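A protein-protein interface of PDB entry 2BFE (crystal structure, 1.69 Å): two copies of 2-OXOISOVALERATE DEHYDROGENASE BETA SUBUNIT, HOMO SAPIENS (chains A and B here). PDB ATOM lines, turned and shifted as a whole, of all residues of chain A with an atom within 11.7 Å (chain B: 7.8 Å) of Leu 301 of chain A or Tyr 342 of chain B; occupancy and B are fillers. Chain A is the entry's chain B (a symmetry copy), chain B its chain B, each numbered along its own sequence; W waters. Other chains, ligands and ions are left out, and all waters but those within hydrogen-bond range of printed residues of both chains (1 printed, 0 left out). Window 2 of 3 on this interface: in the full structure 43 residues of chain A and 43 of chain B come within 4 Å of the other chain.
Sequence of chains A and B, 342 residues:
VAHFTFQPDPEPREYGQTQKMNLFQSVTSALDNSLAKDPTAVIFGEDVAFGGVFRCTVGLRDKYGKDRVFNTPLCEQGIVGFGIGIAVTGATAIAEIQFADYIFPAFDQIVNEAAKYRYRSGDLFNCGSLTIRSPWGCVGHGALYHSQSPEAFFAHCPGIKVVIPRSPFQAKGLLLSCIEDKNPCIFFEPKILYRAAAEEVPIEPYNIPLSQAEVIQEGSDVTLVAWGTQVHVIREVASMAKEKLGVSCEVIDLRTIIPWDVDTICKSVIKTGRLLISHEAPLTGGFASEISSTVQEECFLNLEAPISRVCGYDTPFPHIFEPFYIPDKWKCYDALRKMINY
O of Ser 293 of chain A lies within hydrogen-bond range of NE2 of Gln 296 of chain A, 3.4 Å away.
Gln 296 of chain A touches Pro 306 of chain B (OE1 to CA, 3.2 Å). Phe 300 of chain A touches Leu 303 of chain B. Phe 300 of chain A touches Ala 305 of chain B. Pro 306 of chain B touches Phe 300 of chain A. Tyr 342 of chain B touches Phe 300 of chain A (OH to CB, 3.6 Å). Tyr 342 of chain B touches Leu 301 of chain A.
Printed residues of chain B within 4 Å of Phe 300 of chain A: Leu 303 (3.6 Å), Ala 305 (3.4 Å), Pro 306 (3.7 Å) and Tyr 342 (3.6 Å). Leu 301 of chain A touches one residue of chain B. Of the printed residues of chain A, Leu 303 of chain B touches Phe 300. Printed residues of chain A within 4 Å of Pro 306 of chain B: Gln 296 and Phe 300. Ile 340 of chain B touches none of the printed residues of chain A. No residue of chain A comes within 4 Å of Asn 341 of chain B. Of chain A, only Phe 300 (3.6 Å) and Leu 301 (3.3 Å) come within 4 Å of Tyr 342 of chain B. The nearest printed residue of chain B that does not touch Phe 300 of chain A is Glu 304 of chain B (4.1 Å).
Of the 12 printed residues of chain B, 4 touch a printed residue of chain A. Hydrophobic or aromatic side chains of chain B within 4 Å of the printed part of chain A: Leu 303, Pro 306 and Tyr 342. Of the 25 printed residues of chain A, 3 touch a printed residue of chain B. Hydrophobic or aromatic side chains of chain A within 4 Å of the printed part of chain B: Phe 300 and Leu 301. Among the printed residues, 6 pairs touch across the chains. Among the printed residues, no Asp or Glu carboxylate lies within 4 Å of a Lys or Arg side-chain nitrogen of the other chain.
5 positions are printed for both chains.
Water W1 lies within hydrogen-bond range of the side-chain hydroxyl of Tyr 342 of chain B (2.8 Å) and the backbone carbonyl oxygen of Glu 297 of chain A (2.9 Å).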
ATOM      1  N   CYS A 266      22.999  19.261   7.596  1.00  0.00           N
ATOM      2  CA  CYS A 266      21.814  20.144   7.483  1.00  0.00           C
ATOM      3  C   CYS A 266      21.190  20.417   8.842  1.00  0.00           C
ATOM      4  O   CYS A 266      20.789  21.537   9.125  1.00  0.00           O
ATOM      5  CB  CYS A 266      20.762  19.576   6.506  1.00  0.00           C
ATOM      6  SG  CYS A 266      21.355  19.540   4.794  1.00  0.00           S
ATOM      7  N   SER A 268      22.657  20.709  11.613  1.00  0.00           N
ATOM      8  CA  SER A 268      23.505  21.693  12.285  1.00  0.00           C
ATOM      9  C   SER A 268      23.285  23.086  11.701  1.00  0.00           C
ATOM     10  O   SER A 268      23.189  24.049  12.436  1.00  0.00           O
ATOM     11  CB  SER A 268      24.972  21.291  12.122  1.00  0.00           C
ATOM     12  OG  SER A 268      25.812  22.218  12.770  1.00  0.00           O
ATOM     13  N   VAL A 269      23.242  23.183  10.369  1.00  0.00           N
ATOM     14  CA  VAL A 269      23.045  24.488   9.708  1.00  0.00           C
ATOM     15  C   VAL A 269      21.660  25.087   9.950  1.00  0.00           C
ATOM     16  O   VAL A 269      21.509  26.335  10.104  1.00  0.00           O
ATOM     17  CB  VAL A 269      23.433  24.413   8.194  1.00  0.00           C
ATOM     18  CG1 VAL A 269      23.213  25.790   7.530  1.00  0.00           C
ATOM     19  CG2 VAL A 269      24.915  23.920   8.011  1.00  0.00           C
ATOM     20  N   ILE A 270      20.634  24.234  10.060  1.00  0.00           N
ATOM     21  CA  ILE A 270      19.302  24.754  10.491  1.00  0.00           C
ATOM     22  C   ILE A 270      19.401  25.436  11.858  1.00  0.00           C
ATOM     23  O   ILE A 270      18.742  26.477  12.109  1.00  0.00           O
ATOM     24  CB  ILE A 270      18.234  23.638  10.440  1.00  0.00           C
ATOM     25  CG1 ILE A 270      18.102  23.151   8.978  1.00  0.00           C
ATOM     26  CG2 ILE A 270      16.877  24.101  11.131  1.00  0.00           C
ATOM     27  CD1 ILE A 270      17.391  21.840   8.783  1.00  0.00           C
ATOM     28  N   LYS A 271      20.207  24.873  12.750  1.00  0.00           N
ATOM     29  CA  LYS A 271      20.418  25.453  14.062  1.00  0.00           C
ATOM     30  C   LYS A 271      21.249  26.746  14.043  1.00  0.00           C
ATOM     31  O   LYS A 271      20.866  27.738  14.642  1.00  0.00           O
ATOM     32  CB  LYS A 271      21.090  24.450  15.011  1.00  0.00           C
ATOM     33  CG  LYS A 271      21.412  25.044  16.399  1.00  0.00           C
ATOM     34  CD  LYS A 271      21.928  24.004  17.409  1.00  0.00           C
ATOM     35  CE  LYS A 271      23.233  23.365  16.955  1.00  0.00           C
ATOM     36  NZ  LYS A 271      23.880  22.714  18.125  1.00  0.00           N
ATOM     37  N   THR A 272      22.416  26.713  13.407  1.00  0.00           N
ATOM     38  CA  THR A 272      23.336  27.862  13.468  1.00  0.00           C
ATOM     39  C   THR A 272      23.066  28.944  12.420  1.00  0.00           C
ATOM     40  O   THR A 272      23.313  30.126  12.680  1.00  0.00           O
ATOM     41  CB  THR A 272      24.772  27.416  13.289  1.00  0.00           C
ATOM     42  OG1 THR A 272      24.904  26.846  11.976  1.00  0.00           O
ATOM     43  CG2 THR A 272      25.140  26.304  14.271  1.00  0.00           C
ATOM     44  N   GLY A 273      22.579  28.538  11.249  1.00  0.00           N
ATOM     45  CA  GLY A 273      22.335  29.448  10.154  1.00  0.00           C
ATOM     46  C   GLY A 273      23.546  29.895   9.351  1.00  0.00           C
ATOM     47  O   GLY A 273      23.410  30.730   8.464  1.00  0.00           O
ATOM     48  N   ARG A 274      24.719  29.308   9.617  1.00  0.00           N
ATOM     49  CA  ARG A 274      25.944  29.719   8.939  1.00  0.00           C
ATOM     50  C   ARG A 274      26.931  28.549   8.821  1.00  0.00           C
ATOM     51  O   ARG A 274      27.164  27.856   9.803  1.00  0.00           O
ATOM     52  CB  ARG A 274      26.638  30.868   9.681  1.00  0.00           C
ATOM     53  CG  ARG A 274      25.769  32.087  10.041  1.00  0.00           C
ATOM     54  CD  ARG A 274      26.546  33.200  10.773  1.00  0.00           C
ATOM     55  NE  ARG A 274      25.657  34.248  11.272  1.00  0.00           N
ATOM     56  CZ  ARG A 274      24.914  34.182  12.377  1.00  0.00           C
ATOM     57  NH1 ARG A 274      24.924  33.118  13.173  1.00  0.00           N
ATOM     58  NH2 ARG A 274      24.151  35.218  12.690  1.00  0.00           N
ATOM     59  N   LEU A 275      27.542  28.378   7.640  1.00  0.00           N
ATOM     60  CA  LEU A 275      28.378  27.223   7.366  1.00  0.00           C
ATOM     61  C   LEU A 275      29.665  27.640   6.674  1.00  0.00           C
ATOM     62  O   LEU A 275      29.652  28.408   5.690  1.00  0.00           O
ATOM     63  CB  LEU A 275      27.663  26.250   6.406  1.00  0.00           C
ATOM     64  CG  LEU A 275      28.504  25.064   5.924  1.00  0.00           C
ATOM     65  CD1 LEU A 275      28.939  24.167   7.063  1.00  0.00           C
ATOM     66  CD2 LEU A 275      27.649  24.266   4.901  1.00  0.00           C
ATOM     67  N   SER A 292      28.155  22.529  -0.090  1.00  0.00           N
ATOM     68  CA  SER A 292      27.561  23.875  -0.063  1.00  0.00           C
ATOM     69  C   SER A 292      26.262  23.921  -0.883  1.00  0.00           C
ATOM     70  O   SER A 292      25.268  24.433  -0.428  1.00  0.00           O
ATOM     71  CB  SER A 292      28.560  24.892  -0.664  1.00  0.00           C
ATOM     72  OG  SER A 292      27.948  26.185  -0.745  1.00  0.00           O
ATOM     73  N   SER A 293      26.294  23.370  -2.083  1.00  0.00           N
ATOM     74  CA  SER A 293      25.102  23.423  -2.926  1.00  0.00           C
ATOM     75  C   SER A 293      23.938  22.601  -2.353  1.00  0.00           C
ATOM     76  O   SER A 293      22.782  22.965  -2.550  1.00  0.00           O
ATOM     77  CB  SER A 293      25.443  23.007  -4.362  1.00  0.00           C
ATOM     78  OG  SER A 293      25.959  21.700  -4.398  1.00  0.00           O
ATOM     79  N   THR A 294      24.235  21.501  -1.655  1.00  0.00           N
ATOM     80  CA  THR A 294      23.215  20.675  -1.033  1.00  0.00           C
ATOM     81  C   THR A 294      22.639  21.366   0.188  1.00  0.00           C
ATOM     82  O   THR A 294      21.428  21.407   0.364  1.00  0.00           O
ATOM     83  CB  THR A 294      23.811  19.336  -0.621  1.00  0.00           C
ATOM     84  OG1 THR A 294      24.198  18.637  -1.814  1.00  0.00           O
ATOM     85  CG2 THR A 294      22.798  18.431   0.018  1.00  0.00           C
ATOM     86  N   VAL A 295      23.510  21.912   1.037  1.00  0.00           N
ATOM     87  CA  VAL A 295      23.020  22.633   2.225  1.00  0.00           C
ATOM     88  C   VAL A 295      22.186  23.821   1.818  1.00  0.00           C
ATOM     89  O   VAL A 295      21.172  24.126   2.437  1.00  0.00           O
ATOM     90  CB  VAL A 295      24.188  23.048   3.141  1.00  0.00           C
ATOM     91  CG1 VAL A 295      23.774  24.103   4.202  1.00  0.00           C
ATOM     92  CG2 VAL A 295      24.777  21.785   3.821  1.00  0.00           C
ATOM     93  N   GLN A 296      22.608  24.501   0.758  1.00  0.00           N
ATOM     94  CA  GLN A 296      21.853  25.628   0.222  1.00  0.00           C
ATOM     95  C   GLN A 296      20.430  25.230  -0.207  1.00  0.00           C
ATOM     96  O   GLN A 296      19.460  25.960   0.026  1.00  0.00           O
ATOM     97  CB  GLN A 296      22.637  26.245  -0.939  1.00  0.00           C
ATOM     98  CG  GLN A 296      21.972  27.482  -1.554  1.00  0.00           C
ATOM     99  CD  GLN A 296      21.121  27.153  -2.765  1.00  0.00           C
ATOM    100  OE1 GLN A 296      20.359  27.994  -3.217  1.00  0.00           O
ATOM    101  NE2 GLN A 296      21.255  25.932  -3.296  1.00  0.00           N
ATOM    102  N   GLU A 297      20.302  24.062  -0.819  1.00  0.00           N
ATOM    103  CA  GLU A 297      19.002  23.557  -1.277  1.00  0.00           C
ATOM    104  C   GLU A 297      18.117  23.203  -0.060  1.00  0.00           C
ATOM    105  O   GLU A 297      16.889  23.486  -0.067  1.00  0.00           O
ATOM    106  CB  GLU A 297      19.226  22.301  -2.162  1.00  0.00           C
ATOM    107  CG  GLU A 297      19.731  22.522  -3.590  1.00  0.00           C
ATOM    108  CD  GLU A 297      20.502  21.319  -4.165  1.00  0.00           C
ATOM    109  OE1 GLU A 297      20.602  20.245  -3.520  1.00  0.00           O
ATOM    110  OE2 GLU A 297      21.100  21.468  -5.254  1.00  0.00           O
ATOM    111  N   GLU A 298      18.709  22.583   0.959  1.00  0.00           N
ATOM    112  CA  GLU A 298      17.938  22.034   2.080  1.00  0.00           C
ATOM    113  C   GLU A 298      17.690  23.039   3.214  1.00  0.00           C
ATOM    114  O   GLU A 298      16.701  22.922   3.970  1.00  0.00           O
ATOM    115  CB  GLU A 298      18.629  20.782   2.643  1.00  0.00           C
ATOM    116  CG  GLU A 298      18.717  19.595   1.665  1.00  0.00           C
ATOM    117  CD  GLU A 298      17.345  19.267   1.080  1.00  0.00           C
ATOM    118  OE1 GLU A 298      16.367  19.227   1.887  1.00  0.00           O
ATOM    119  OE2 GLU A 298      17.225  19.107  -0.166  1.00  0.00           O
ATOM    120  N   CYS A 299      18.582  24.024   3.341  1.00  0.00           N
ATOM    121  CA  CYS A 299      18.554  24.983   4.452  1.00  0.00           C
ATOM    122  C   CYS A 299      18.429  26.421   3.995  1.00  0.00           C
ATOM    123  O   CYS A 299      18.710  27.327   4.772  1.00  0.00           O
ATOM    124  CB  CYS A 299      19.837  24.859   5.278  1.00  0.00           C
ATOM    125  SG  CYS A 299      20.166  23.139   5.750  1.00  0.00           S
ATOM    126  N   PHE A 300      18.018  26.634   2.748  1.00  0.00           N
ATOM    127  CA  PHE A 300      17.938  27.977   2.165  1.00  0.00           C
ATOM    128  C   PHE A 300      17.359  29.032   3.110  1.00  0.00           C
ATOM    129  O   PHE A 300      17.971  30.073   3.327  1.00  0.00           O
ATOM    130  CB  PHE A 300      17.060  27.945   0.915  1.00  0.00           C
ATOM    131  CG  PHE A 300      17.134  29.193   0.084  1.00  0.00           C
ATOM    132  CD1 PHE A 300      18.301  29.517  -0.644  1.00  0.00           C
ATOM    133  CD2 PHE A 300      16.032  30.019  -0.022  1.00  0.00           C
ATOM    134  CE1 PHE A 300      18.348  30.668  -1.455  1.00  0.00           C
ATOM    135  CE2 PHE A 300      16.073  31.166  -0.819  1.00  0.00           C
ATOM    136  CZ  PHE A 300      17.222  31.515  -1.504  1.00  0.00           C
ATOM    137  N   LEU A 301      16.189  28.754   3.659  1.00  0.00           N
ATOM    138  CA  LEU A 301      15.526  29.749   4.471  1.00  0.00           C
ATOM    139  C   LEU A 301      16.198  30.020   5.818  1.00  0.00           C
ATOM    140  O   LEU A 301      15.803  30.957   6.516  1.00  0.00           O
ATOM    141  CB  LEU A 301      14.065  29.352   4.670  1.00  0.00           C
ATOM    142  CG  LEU A 301      13.117  29.436   3.466  1.00  0.00           C
ATOM    143  CD1 LEU A 301      11.736  29.015   3.877  1.00  0.00           C
ATOM    144  CD2 LEU A 301      13.026  30.861   2.872  1.00  0.00           C
ATOM    145  N   ASN A 302      17.189  29.218   6.195  1.00  0.00           N
ATOM    146  CA  ASN A 302      17.870  29.379   7.482  1.00  0.00           C
ATOM    147  C   ASN A 302      19.192  30.114   7.338  1.00  0.00           C
ATOM    148  O   ASN A 302      19.833  30.445   8.337  1.00  0.00           O
ATOM    149  CB  ASN A 302      18.193  28.015   8.060  1.00  0.00           C
ATOM    150  CG  ASN A 302      16.999  27.114   8.096  1.00  0.00           C
ATOM    151  OD1 ASN A 302      16.901  26.162   7.311  1.00  0.00           O
ATOM    152  ND2 ASN A 302      16.101  27.380   9.015  1.00  0.00           N
ATOM    153  N   LEU A 303      19.628  30.334   6.097  1.00  0.00           N
ATOM    154  CA  LEU A 303      20.956  30.846   5.876  1.00  0.00           C
ATOM    155  C   LEU A 303      21.091  32.328   6.119  1.00  0.00           C
ATOM    156  O   LEU A 303      20.426  33.138   5.453  1.00  0.00           O
ATOM    157  CB  LEU A 303      21.447  30.503   4.455  1.00  0.00           C
ATOM    158  CG  LEU A 303      21.885  29.085   4.167  1.00  0.00           C
ATOM    159  CD1 LEU A 303      22.258  28.959   2.664  1.00  0.00           C
ATOM    160  CD2 LEU A 303      23.088  28.660   4.999  1.00  0.00           C
ATOM    161  N   GLU A 304      21.935  32.701   7.084  1.00  0.00           N
ATOM    162  CA  GLU A 304      22.067  34.112   7.480  1.00  0.00           C
ATOM    163  C   GLU A 304      23.131  34.831   6.663  1.00  0.00           C
ATOM    164  O   GLU A 304      23.180  36.077   6.676  1.00  0.00           O
ATOM    165  CB  GLU A 304      22.484  34.217   8.964  1.00  0.00           C
ATOM    166  CG  GLU A 304      21.514  33.573   9.922  1.00  0.00           C
ATOM    167  CD  GLU A 304      20.496  34.560  10.385  1.00  0.00           C
ATOM    168  OE1 GLU A 304      20.518  35.726   9.901  1.00  0.00           O
ATOM    169  OE2 GLU A 304      19.666  34.184  11.239  1.00  0.00           O
ATOM    170  N   ALA A 305      24.022  34.039   6.041  1.00  0.00           N
ATOM    171  CA  ALA A 305      25.204  34.531   5.345  1.00  0.00           C
ATOM    172  C   ALA A 305      25.522  33.478   4.279  1.00  0.00           C
ATOM    173  O   ALA A 305      25.118  32.290   4.419  1.00  0.00           O
ATOM    174  CB  ALA A 305      26.393  34.648   6.305  1.00  0.00           C
ATOM    175  N   PRO A 306      26.243  33.851   3.210  1.00  0.00           N
ATOM    176  CA  PRO A 306      26.635  32.864   2.227  1.00  0.00           C
ATOM    177  C   PRO A 306      27.504  31.768   2.847  1.00  0.00           C
ATOM    178  O   PRO A 306      28.319  32.028   3.754  1.00  0.00           O
ATOM    179  CB  PRO A 306      27.489  33.658   1.212  1.00  0.00           C
ATOM    180  CG  PRO A 306      27.285  35.050   1.490  1.00  0.00           C
ATOM    181  CD  PRO A 306      26.745  35.181   2.864  1.00  0.00           C
ATOM    182  N   ILE A 307      27.309  30.546   2.370  1.00  0.00           N
ATOM    183  CA  ILE A 307      28.163  29.447   2.803  1.00  0.00           C
ATOM    184  C   ILE A 307      29.590  29.705   2.292  1.00  0.00           C
ATOM    185  O   ILE A 307      29.783  29.996   1.078  1.00  0.00           O
ATOM    186  CB  ILE A 307      27.617  28.098   2.306  1.00  0.00           C
ATOM    187  CG1 ILE A 307      26.247  27.832   2.892  1.00  0.00           C
ATOM    188  CG2 ILE A 307      28.602  26.939   2.586  1.00  0.00           C
ATOM    189  CD1 ILE A 307      25.544  26.659   2.168  1.00  0.00           C
ATOM    190  N   ARG B 274      17.019  33.857  -9.786  1.00  0.00           N
ATOM    191  CA  ARG B 274      16.718  32.431  -9.714  1.00  0.00           C
ATOM    192  C   ARG B 274      17.514  31.642 -10.762  1.00  0.00           C
ATOM    193  O   ARG B 274      17.549  32.042 -11.919  1.00  0.00           O
ATOM    194  CB  ARG B 274      15.224  32.160  -9.932  1.00  0.00           C
ATOM    195  CG  ARG B 274      14.238  32.980  -9.078  1.00  0.00           C
ATOM    196  CD  ARG B 274      12.760  32.637  -9.351  1.00  0.00           C
ATOM    197  NE  ARG B 274      11.852  33.563  -8.674  1.00  0.00           N
ATOM    198  CZ  ARG B 274      11.537  34.791  -9.088  1.00  0.00           C
ATOM    199  NH1 ARG B 274      12.027  35.306 -10.210  1.00  0.00           N
ATOM    200  NH2 ARG B 274      10.702  35.510  -8.354  1.00  0.00           N
ATOM    201  N   LEU B 303      19.138  36.095  -4.322  1.00  0.00           N
ATOM    202  CA  LEU B 303      18.501  34.824  -4.553  1.00  0.00           C
ATOM    203  C   LEU B 303      17.113  34.720  -3.975  1.00  0.00           C
ATOM    204  O   LEU B 303      16.929  34.843  -2.754  1.00  0.00           O
ATOM    205  CB  LEU B 303      19.375  33.669  -4.025  1.00  0.00           C
ATOM    206  CG  LEU B 303      20.595  33.265  -4.822  1.00  0.00           C
ATOM    207  CD1 LEU B 303      21.357  32.145  -4.062  1.00  0.00           C
ATOM    208  CD2 LEU B 303      20.246  32.752  -6.213  1.00  0.00           C
ATOM    209  N   GLU B 304      16.119  34.511  -4.843  1.00  0.00           N
ATOM    210  CA  GLU B 304      14.714  34.499  -4.406  1.00  0.00           C
ATOM    211  C   GLU B 304      14.264  33.105  -3.991  1.00  0.00           C
ATOM    212  O   GLU B 304      13.206  32.967  -3.344  1.00  0.00           O
ATOM    213  CB  GLU B 304      13.789  34.952  -5.557  1.00  0.00           C
ATOM    214  CG  GLU B 304      14.084  36.337  -6.073  1.00  0.00           C
ATOM    215  CD  GLU B 304      13.276  37.356  -5.342  1.00  0.00           C
ATOM    216  OE1 GLU B 304      12.539  36.976  -4.389  1.00  0.00           O
ATOM    217  OE2 GLU B 304      13.365  38.546  -5.711  1.00  0.00           O
ATOM    218  N   ALA B 305      15.018  32.090  -4.446  1.00  0.00           N
ATOM    219  CA  ALA B 305      14.669  30.683  -4.295  1.00  0.00           C
ATOM    220  C   ALA B 305      16.000  29.924  -4.308  1.00  0.00           C
ATOM    221  O   ALA B 305      17.018  30.438  -4.849  1.00  0.00           O
ATOM    222  CB  ALA B 305      13.809  30.205  -5.469  1.00  0.00           C
ATOM    223  N   PRO B 306      16.046  28.709  -3.740  1.00  0.00           N
ATOM    224  CA  PRO B 306      17.263  27.928  -3.810  1.00  0.00           C
ATOM    225  C   PRO B 306      17.660  27.635  -5.259  1.00  0.00           C
ATOM    226  O   PRO B 306      16.796  27.428  -6.133  1.00  0.00           O
ATOM    227  CB  PRO B 306      16.899  26.596  -3.116  1.00  0.00           C
ATOM    228  CG  PRO B 306      15.649  26.800  -2.442  1.00  0.00           C
ATOM    229  CD  PRO B 306      14.989  27.990  -3.030  1.00  0.00           C
ATOM    230  N   LEU B 336      11.639  23.688 -12.418  1.00  0.00           N
ATOM    231  CA  LEU B 336      11.459  25.116 -12.639  1.00  0.00           C
ATOM    232  C   LEU B 336      10.159  25.621 -12.038  1.00  0.00           C
ATOM    233  O   LEU B 336      10.129  26.707 -11.445  1.00  0.00           O
ATOM    234  CB  LEU B 336      11.467  25.419 -14.129  1.00  0.00           C
ATOM    235  CG  LEU B 336      11.321  26.870 -14.612  1.00  0.00           C
ATOM    236  CD1 LEU B 336      12.234  27.768 -13.828  1.00  0.00           C
ATOM    237  CD2 LEU B 336      11.681  26.942 -16.093  1.00  0.00           C
ATOM    238  N   ARG B 337       9.089  24.840 -12.236  1.00  0.00           N
ATOM    239  CA  ARG B 337       7.747  25.159 -11.707  1.00  0.00           C
ATOM    240  C   ARG B 337       7.793  25.320 -10.176  1.00  0.00           C
ATOM    241  O   ARG B 337       7.275  26.310  -9.619  1.00  0.00           O
ATOM    242  CB  ARG B 337       6.753  24.061 -12.157  1.00  0.00           C
ATOM    243  CG  ARG B 337       5.290  24.353 -11.902  1.00  0.00           C
ATOM    244  CD  ARG B 337       4.371  23.113 -12.088  1.00  0.00           C
ATOM    245  NE  ARG B 337       4.876  21.964 -11.316  1.00  0.00           N
ATOM    246  CZ  ARG B 337       4.692  21.759 -10.003  1.00  0.00           C
ATOM    247  NH1 ARG B 337       3.979  22.618  -9.260  1.00  0.00           N
ATOM    248  NH2 ARG B 337       5.239  20.694  -9.423  1.00  0.00           N
ATOM    249  N   LYS B 338       8.409  24.347  -9.502  1.00  0.00           N
ATOM    250  CA  LYS B 338       8.543  24.404  -8.044  1.00  0.00           C
ATOM    251  C   LYS B 338       9.362  25.616  -7.579  1.00  0.00           C
ATOM    252  O   LYS B 338       9.011  26.259  -6.595  1.00  0.00           O
ATOM    253  CB  LYS B 338       9.175  23.124  -7.505  1.00  0.00           C
ATOM    254  CG  LYS B 338       8.325  21.891  -7.702  1.00  0.00           C
ATOM    255  CD  LYS B 338       9.188  20.709  -7.325  1.00  0.00           C
ATOM    256  CE  LYS B 338       8.496  19.381  -7.580  1.00  0.00           C
ATOM    257  NZ  LYS B 338       9.455  18.293  -7.225  1.00  0.00           N
ATOM    258  N   MET B 339      10.434  25.921  -8.307  1.00  0.00           N
ATOM    259  CA  MET B 339      11.304  27.044  -7.991  1.00  0.00           C
ATOM    260  C   MET B 339      10.575  28.366  -8.118  1.00  0.00           C
ATOM    261  O   MET B 339      10.729  29.220  -7.261  1.00  0.00           O
ATOM    262  CB  MET B 339      12.573  27.015  -8.869  1.00  0.00           C
ATOM    263  CG  MET B 339      13.722  27.810  -8.264  1.00  0.00           C
ATOM    264  SD  MET B 339      15.267  27.588  -9.169  1.00  0.00           S
ATOM    265  CE  MET B 339      14.773  28.233 -10.768  1.00  0.00           C
ATOM    266  N   ILE B 340       9.783  28.535  -9.183  1.00  0.00           N
ATOM    267  CA  ILE B 340       8.918  29.732  -9.371  1.00  0.00           C
ATOM    268  C   ILE B 340       7.913  29.880  -8.230  1.00  0.00           C
ATOM    269  O   ILE B 340       7.554  31.008  -7.857  1.00  0.00           O
ATOM    270  CB  ILE B 340       8.187  29.670 -10.758  1.00  0.00           C
ATOM    271  CG1 ILE B 340       9.177  29.893 -11.906  1.00  0.00           C
ATOM    272  CG2 ILE B 340       7.055  30.654 -10.846  1.00  0.00           C
ATOM    273  CD1 ILE B 340      10.183  31.009 -11.662  1.00  0.00           C
ATOM    274  N   ASN B 341       7.484  28.754  -7.665  1.00  0.00           N
ATOM    275  CA  ASN B 341       6.462  28.744  -6.606  1.00  0.00           C
ATOM    276  C   ASN B 341       7.011  28.779  -5.181  1.00  0.00           C
ATOM    277  O   ASN B 341       6.230  28.848  -4.220  1.00  0.00           O
ATOM    278  CB  ASN B 341       5.565  27.513  -6.766  1.00  0.00           C
ATOM    279  CG  ASN B 341       4.715  27.576  -8.022  1.00  0.00           C
ATOM    280  OD1 ASN B 341       4.315  28.660  -8.463  1.00  0.00           O
ATOM    281  ND2 ASN B 341       4.410  26.418  -8.589  1.00  0.00           N
ATOM    282  N   TYR B 342       8.335  28.776  -5.045  1.00  0.00           N
ATOM    283  CA  TYR B 342       9.001  28.596  -3.742  1.00  0.00           C
ATOM    284  C   TYR B 342       8.551  29.602  -2.690  1.00  0.00           C
ATOM    285  O   TYR B 342       8.623  30.817  -2.921  1.00  0.00           O
ATOM    286  CB  TYR B 342      10.535  28.636  -3.901  1.00  0.00           C
ATOM    287  CG  TYR B 342      11.304  28.327  -2.634  1.00  0.00           C
ATOM    288  CD1 TYR B 342      11.747  29.350  -1.788  1.00  0.00           C
ATOM    289  CD2 TYR B 342      11.625  27.019  -2.305  1.00  0.00           C
ATOM    290  CE1 TYR B 342      12.468  29.071  -0.615  1.00  0.00           C
ATOM    291  CE2 TYR B 342      12.356  26.718  -1.166  1.00  0.00           C
ATOM    292  CZ  TYR B 342      12.762  27.750  -0.295  1.00  0.00           C
ATOM    293  OH  TYR B 342      13.499  27.410   0.850  1.00  0.00           O
ATOM    294  OXT TYR B 342       8.107  29.186  -1.601  1.00  0.00           O
HETATM  295  O   HOH W   1      14.693  24.848   1.179  1.00  0.00           O
